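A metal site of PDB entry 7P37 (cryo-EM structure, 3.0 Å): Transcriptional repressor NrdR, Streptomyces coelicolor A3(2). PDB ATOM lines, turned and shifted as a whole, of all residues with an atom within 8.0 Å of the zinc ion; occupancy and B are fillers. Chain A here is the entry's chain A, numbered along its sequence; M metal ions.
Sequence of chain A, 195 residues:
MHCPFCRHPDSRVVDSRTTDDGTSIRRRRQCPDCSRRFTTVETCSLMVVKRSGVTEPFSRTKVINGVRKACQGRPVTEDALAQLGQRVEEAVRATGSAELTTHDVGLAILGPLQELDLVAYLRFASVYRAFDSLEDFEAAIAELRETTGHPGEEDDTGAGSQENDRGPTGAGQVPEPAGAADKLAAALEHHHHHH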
ATOM      1  N   MET A   1     -20.975 -14.281  33.078  1.00  0.00           N
ATOM      2  CA  MET A   1     -21.150 -15.639  32.584  1.00  0.00           C
ATOM      3  C   MET A   1     -20.534 -15.808  31.194  1.00  0.00           C
ATOM      4  O   MET A   1     -20.483 -14.863  30.413  1.00  0.00           O
ATOM      5  CB  MET A   1     -22.635 -16.001  32.544  1.00  0.00           C
ATOM      6  CG  MET A   1     -22.919 -17.477  32.743  1.00  0.00           C
ATOM      7  SD  MET A   1     -24.676 -17.866  32.681  1.00  0.00           S
ATOM      8  CE  MET A   1     -24.983 -17.695  30.932  1.00  0.00           C
ATOM      9  N   HIS A   2     -20.058 -17.015  30.903  1.00  0.00           N
ATOM     10  CA  HIS A   2     -19.470 -17.294  29.607  1.00  0.00           C
ATOM     11  C   HIS A   2     -20.529 -17.276  28.508  1.00  0.00           C
ATOM     12  O   HIS A   2     -21.629 -17.802  28.680  1.00  0.00           O
ATOM     13  CB  HIS A   2     -18.751 -18.647  29.628  1.00  0.00           C
ATOM     14  CG  HIS A   2     -17.379 -18.591  30.234  1.00  0.00           C
ATOM     15  ND1 HIS A   2     -16.268 -18.167  29.534  1.00  0.00           N
ATOM     16  CD2 HIS A   2     -16.952 -18.902  31.476  1.00  0.00           C
ATOM     17  CE1 HIS A   2     -15.216 -18.231  30.321  1.00  0.00           C
ATOM     18  NE2 HIS A   2     -15.600 -18.665  31.506  1.00  0.00           N
ATOM     19  N   CYS A   3     -20.191 -16.671  27.389  1.00  0.00           N
ATOM     20  CA  CYS A   3     -21.098 -16.631  26.251  1.00  0.00           C
ATOM     21  C   CYS A   3     -21.268 -18.040  25.686  1.00  0.00           C
ATOM     22  O   CYS A   3     -20.272 -18.729  25.439  1.00  0.00           O
ATOM     23  CB  CYS A   3     -20.565 -15.692  25.175  1.00  0.00           C
ATOM     24  SG  CYS A   3     -21.541 -15.638  23.654  1.00  0.00           S
ATOM     25  N   PRO A   4     -22.499 -18.499  25.475  1.00  0.00           N
ATOM     26  CA  PRO A   4     -22.694 -19.869  24.977  1.00  0.00           C
ATOM     27  C   PRO A   4     -22.088 -20.119  23.606  1.00  0.00           C
ATOM     28  O   PRO A   4     -21.743 -21.256  23.282  1.00  0.00           O
ATOM     29  CB  PRO A   4     -24.221 -20.019  24.935  1.00  0.00           C
ATOM     30  CG  PRO A   4     -24.733 -18.962  25.860  1.00  0.00           C
ATOM     31  CD  PRO A   4     -23.784 -17.826  25.745  1.00  0.00           C
ATOM     32  N   PHE A   5     -21.930 -19.075  22.784  1.00  0.00           N
ATOM     33  CA  PHE A   5     -21.487 -19.242  21.406  1.00  0.00           C
ATOM     34  C   PHE A   5     -19.970 -19.148  21.265  1.00  0.00           C
ATOM     35  O   PHE A   5     -19.355 -19.995  20.610  1.00  0.00           O
ATOM     36  CB  PHE A   5     -22.181 -18.214  20.513  1.00  0.00           C
ATOM     37  CG  PHE A   5     -23.634 -18.033  20.806  1.00  0.00           C
ATOM     38  CD1 PHE A   5     -24.554 -19.009  20.438  1.00  0.00           C
ATOM     39  CD2 PHE A   5     -24.094 -16.898  21.448  1.00  0.00           C
ATOM     40  CE1 PHE A   5     -25.899 -18.838  20.715  1.00  0.00           C
ATOM     41  CE2 PHE A   5     -25.434 -16.724  21.716  1.00  0.00           C
ATOM     42  CZ  PHE A   5     -26.342 -17.703  21.355  1.00  0.00           C
ATOM     43  N   CYS A   6     -19.353 -18.127  21.863  1.00  0.00           N
ATOM     44  CA  CYS A   6     -17.937 -17.882  21.696  1.00  0.00           C
ATOM     45  C   CYS A   6     -17.128 -18.082  22.977  1.00  0.00           C
ATOM     46  O   CYS A   6     -15.907 -17.870  22.955  1.00  0.00           O
ATOM     47  CB  CYS A   6     -17.700 -16.464  21.156  1.00  0.00           C
ATOM     48  SG  CYS A   6     -17.971 -15.166  22.371  1.00  0.00           S
ATOM     49  N   ARG A   7     -17.770 -18.480  24.077  1.00  0.00           N
ATOM     50  CA  ARG A   7     -17.088 -18.777  25.337  1.00  0.00           C
ATOM     51  C   ARG A   7     -16.270 -17.590  25.855  1.00  0.00           C
ATOM     52  O   ARG A   7     -15.181 -17.770  26.398  1.00  0.00           O
ATOM     53  CB  ARG A   7     -16.203 -20.019  25.207  1.00  0.00           C
ATOM     54  CG  ARG A   7     -16.933 -21.259  24.742  1.00  0.00           C
ATOM     55  CD  ARG A   7     -17.830 -21.817  25.830  1.00  0.00           C
ATOM     56  NE  ARG A   7     -17.084 -22.175  27.025  1.00  0.00           N
ATOM     57  CZ  ARG A   7     -16.574 -23.381  27.266  1.00  0.00           C
ATOM     58  NH1 ARG A   7     -16.723 -24.370  26.395  1.00  0.00           N
ATOM     59  NH2 ARG A   7     -15.900 -23.591  28.388  1.00  0.00           N
ATOM     60  N   HIS A   8     -16.782 -16.377  25.679  1.00  0.00           N
ATOM     61  CA  HIS A   8     -16.103 -15.201  26.197  1.00  0.00           C
ATOM     62  C   HIS A   8     -16.123 -15.229  27.733  1.00  0.00           C
ATOM     63  O   HIS A   8     -17.093 -15.708  28.328  1.00  0.00           O
ATOM     64  CB  HIS A   8     -16.770 -13.926  25.685  1.00  0.00           C
ATOM     65  CG  HIS A   8     -15.941 -12.696  25.842  1.00  0.00           C
ATOM     66  ND1 HIS A   8     -16.220 -11.723  26.778  1.00  0.00           N
ATOM     67  CD2 HIS A   8     -14.823 -12.282  25.191  1.00  0.00           C
ATOM     68  CE1 HIS A   8     -15.316 -10.766  26.690  1.00  0.00           C
ATOM     69  NE2 HIS A   8     -14.454 -11.076  25.741  1.00  0.00           N
ATOM     70  N   PRO A   9     -15.068 -14.738  28.392  1.00  0.00           N
ATOM     71  CA  PRO A   9     -15.017 -14.836  29.862  1.00  0.00           C
ATOM     72  C   PRO A   9     -16.170 -14.151  30.577  1.00  0.00           C
ATOM     73  O   PRO A   9     -16.604 -14.647  31.627  1.00  0.00           O
ATOM     74  CB  PRO A   9     -13.674 -14.177  30.206  1.00  0.00           C
ATOM     75  CG  PRO A   9     -13.269 -13.422  28.971  1.00  0.00           C
ATOM     76  CD  PRO A   9     -13.811 -14.212  27.838  1.00  0.00           C
ATOM     77  N   ASP A  10     -16.687 -13.029  30.069  1.00  0.00           N
ATOM     78  CA  ASP A  10     -17.738 -12.298  30.751  1.00  0.00           C
ATOM     79  C   ASP A  10     -18.754 -11.773  29.762  1.00  0.00           C
ATOM     80  O   ASP A  10     -18.456 -11.603  28.580  1.00  0.00           O
ATOM     81  CB  ASP A  10     -17.159 -11.136  31.579  1.00  0.00           C
ATOM     82  CG  ASP A  10     -16.428 -10.125  30.728  1.00  0.00           C
ATOM     83  OD1 ASP A  10     -15.797 -10.528  29.739  1.00  0.00           O
ATOM     84  OD2 ASP A  10     -16.491  -8.919  31.050  1.00  0.00           O
ATOM     85  N   SER A  11     -19.965 -11.513  30.258  1.00  0.00           N
ATOM     86  CA  SER A  11     -21.039 -10.943  29.455  1.00  0.00           C
ATOM     87  C   SER A  11     -21.788  -9.908  30.281  1.00  0.00           C
ATOM     88  O   SER A  11     -21.736  -9.916  31.518  1.00  0.00           O
ATOM     89  CB  SER A  11     -22.005 -12.038  28.956  1.00  0.00           C
ATOM     90  OG  SER A  11     -22.470 -12.834  30.037  1.00  0.00           O
ATOM     91  N   GLN A  30     -26.023  -9.927  26.802  1.00  0.00           N
ATOM     92  CA  GLN A  30     -25.385  -9.701  25.508  1.00  0.00           C
ATOM     93  C   GLN A  30     -23.880  -9.816  25.663  1.00  0.00           C
ATOM     94  O   GLN A  30     -23.299  -9.227  26.576  1.00  0.00           O
ATOM     95  CB  GLN A  30     -25.760  -8.321  24.940  1.00  0.00           C
ATOM     96  CG  GLN A  30     -25.016  -7.952  23.675  1.00  0.00           C
ATOM     97  CD  GLN A  30     -25.599  -6.730  22.988  1.00  0.00           C
ATOM     98  OE1 GLN A  30     -26.710  -6.294  23.311  1.00  0.00           O
ATOM     99  NE2 GLN A  30     -24.855  -6.176  22.045  1.00  0.00           N
ATOM    100  N   CYS A  31     -23.258 -10.570  24.767  1.00  0.00           N
ATOM    101  CA  CYS A  31     -21.801 -10.734  24.810  1.00  0.00           C
ATOM    102  C   CYS A  31     -21.122  -9.499  24.245  1.00  0.00           C
ATOM    103  O   CYS A  31     -21.472  -9.060  23.144  1.00  0.00           O
ATOM    104  CB  CYS A  31     -21.376 -11.968  24.027  1.00  0.00           C
ATOM    105  SG  CYS A  31     -19.624 -12.351  24.190  1.00  0.00           S
ATOM    106  N   PRO A  32     -20.172  -8.902  24.966  1.00  0.00           N
ATOM    107  CA  PRO A  32     -19.525  -7.679  24.464  1.00  0.00           C
ATOM    108  C   PRO A  32     -18.786  -7.868  23.149  1.00  0.00           C
ATOM    109  O   PRO A  32     -18.727  -6.928  22.346  1.00  0.00           O
ATOM    110  CB  PRO A  32     -18.569  -7.299  25.600  1.00  0.00           C
ATOM    111  CG  PRO A  32     -18.334  -8.567  26.349  1.00  0.00           C
ATOM    112  CD  PRO A  32     -19.611  -9.331  26.257  1.00  0.00           C
ATOM    113  N   ASP A  33     -18.209  -9.045  22.906  1.00  0.00           N
ATOM    114  CA  ASP A  33     -17.387  -9.234  21.715  1.00  0.00           C
ATOM    115  C   ASP A  33     -18.227  -9.554  20.487  1.00  0.00           C
ATOM    116  O   ASP A  33     -18.238  -8.796  19.508  1.00  0.00           O
ATOM    117  CB  ASP A  33     -16.355 -10.340  21.958  1.00  0.00           C
ATOM    118  CG  ASP A  33     -15.278  -9.927  22.931  1.00  0.00           C
ATOM    119  OD1 ASP A  33     -15.558  -9.060  23.792  1.00  0.00           O
ATOM    120  OD2 ASP A  33     -14.146 -10.460  22.837  1.00  0.00           O
ATOM    121  N   CYS A  34     -18.950 -10.675  20.518  1.00  0.00           N
ATOM    122  CA  CYS A  34     -19.696 -11.129  19.346  1.00  0.00           C
ATOM    123  C   CYS A  34     -21.060 -10.460  19.205  1.00  0.00           C
ATOM    124  O   CYS A  34     -21.736 -10.696  18.200  1.00  0.00           O
ATOM    125  CB  CYS A  34     -19.859 -12.646  19.385  1.00  0.00           C
ATOM    126  SG  CYS A  34     -20.873 -13.265  20.750  1.00  0.00           S
ATOM    127  N   SER A  35     -21.435  -9.616  20.175  1.00  0.00           N
ATOM    128  CA  SER A  35     -22.767  -8.921  20.164  1.00  0.00           C
ATOM    129  C   SER A  35     -23.895  -9.937  19.930  1.00  0.00           C
ATOM    130  O   SER A  35     -24.675  -9.750  18.961  1.00  0.00           O
ATOM    131  CB  SER A  35     -22.799  -7.732  19.223  1.00  0.00           C
ATOM    132  OG  SER A  35     -22.708  -8.114  17.863  1.00  0.00           O
ATOM    133  N   ARG A  36     -23.985 -10.961  20.777  1.00  0.00           N
ATOM    134  CA  ARG A  36     -25.061 -11.998  20.665  1.00  0.00           C
ATOM    135  C   ARG A  36     -25.889 -12.002  21.950  1.00  0.00           C
ATOM    136  O   ARG A  36     -25.281 -12.011  23.039  1.00  0.00           O
ATOM    137  CB  ARG A  36     -24.475 -13.373  20.385  1.00  0.00           C
ATOM    138  CG  ARG A  36     -24.122 -13.632  18.924  1.00  0.00           C
ATOM    139  CD  ARG A  36     -25.350 -13.595  18.021  1.00  0.00           C
ATOM    140  NE  ARG A  36     -26.351 -14.586  18.361  1.00  0.00           N
ATOM    141  CZ  ARG A  36     -26.401 -15.823  17.871  1.00  0.00           C
ATOM    142  NH1 ARG A  36     -25.488 -16.248  17.012  1.00  0.00           N
ATOM    143  NH2 ARG A  36     -27.370 -16.637  18.249  1.00  0.00           N
ATOM    144  N   ARG A  37     -27.223 -12.039  21.825  1.00  0.00           N
ATOM    145  CA  ARG A  37     -28.088 -11.930  23.040  1.00  0.00           C
ATOM    146  C   ARG A  37     -28.673 -13.306  23.395  1.00  0.00           C
ATOM    147  O   ARG A  37     -29.231 -13.965  22.489  1.00  0.00           O
ATOM    148  CB  ARG A  37     -29.182 -10.879  22.822  1.00  0.00           C
ATOM    149  CG  ARG A  37     -28.691  -9.439  22.915  1.00  0.00           C
ATOM    150  CD  ARG A  37     -29.248  -8.594  21.794  1.00  0.00           C
ATOM    151  NE  ARG A  37     -28.983  -9.189  20.488  1.00  0.00           N
ATOM    152  CZ  ARG A  37     -27.900  -8.963  19.743  1.00  0.00           C
ATOM    153  NH1 ARG A  37     -26.962  -8.124  20.170  1.00  0.00           N
ATOM    154  NH2 ARG A  37     -27.759  -9.566  18.585  1.00  0.00           N
ATOM    155  N   PHE A  38     -28.548 -13.715  24.666  1.00  0.00           N
ATOM    156  CA  PHE A  38     -28.996 -15.064  25.114  1.00  0.00           C
ATOM    157  C   PHE A  38     -29.813 -14.941  26.414  1.00  0.00           C
ATOM    158  O   PHE A  38     -29.593 -13.982  27.175  1.00  0.00           O
ATOM    159  CB  PHE A  38     -27.790 -15.988  25.281  1.00  0.00           C
ATOM    160  CG  PHE A  38     -26.590 -15.388  25.964  1.00  0.00           C
ATOM    161  CD1 PHE A  38     -25.633 -14.680  25.255  1.00  0.00           C
ATOM    162  CD2 PHE A  38     -26.392 -15.560  27.336  1.00  0.00           C
ATOM    163  CE1 PHE A  38     -24.534 -14.134  25.890  1.00  0.00           C
ATOM    164  CE2 PHE A  38     -25.282 -15.018  27.963  1.00  0.00           C
ATOM    165  CZ  PHE A  38     -24.357 -14.307  27.237  1.00  0.00           C
HETATM  166 ZN    ZN M   1     -20.022 -14.124  22.736  1.00  0.00          ZN
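The zinc ion is bound by SG of Cys 34 (2.3 Å), SG of Cys 31 (2.3 Å), SG of Cys 6 (2.3 Å) and SG of Cys 3 (2.3 Å). The zinc ion has four donor atoms within binding distance.
The backbone NH (N) of Cys 3 lies within hydrogen-bond range of the backbone carbonyl oxygen (O) of His 8 (3.4 Å). The backbone NH of Cys 31 sits at hydrogen-bond distance from the backbone carbonyl oxygen of Arg 36 (3.0 Å). The side-chain sulfur (SG) of Cys 3 lies close to the backbone NH (N) of Phe 5, at 3.6 Å. The side-chain sulfur (SG) of Cys 6 lies close to the backbone NH (N) of His 8.
Of the 20 residues printed, 4 come within 4 Å of the zinc ion. The nearest printed residue that does not touch the zinc ion is His 8 (4.4 Å).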
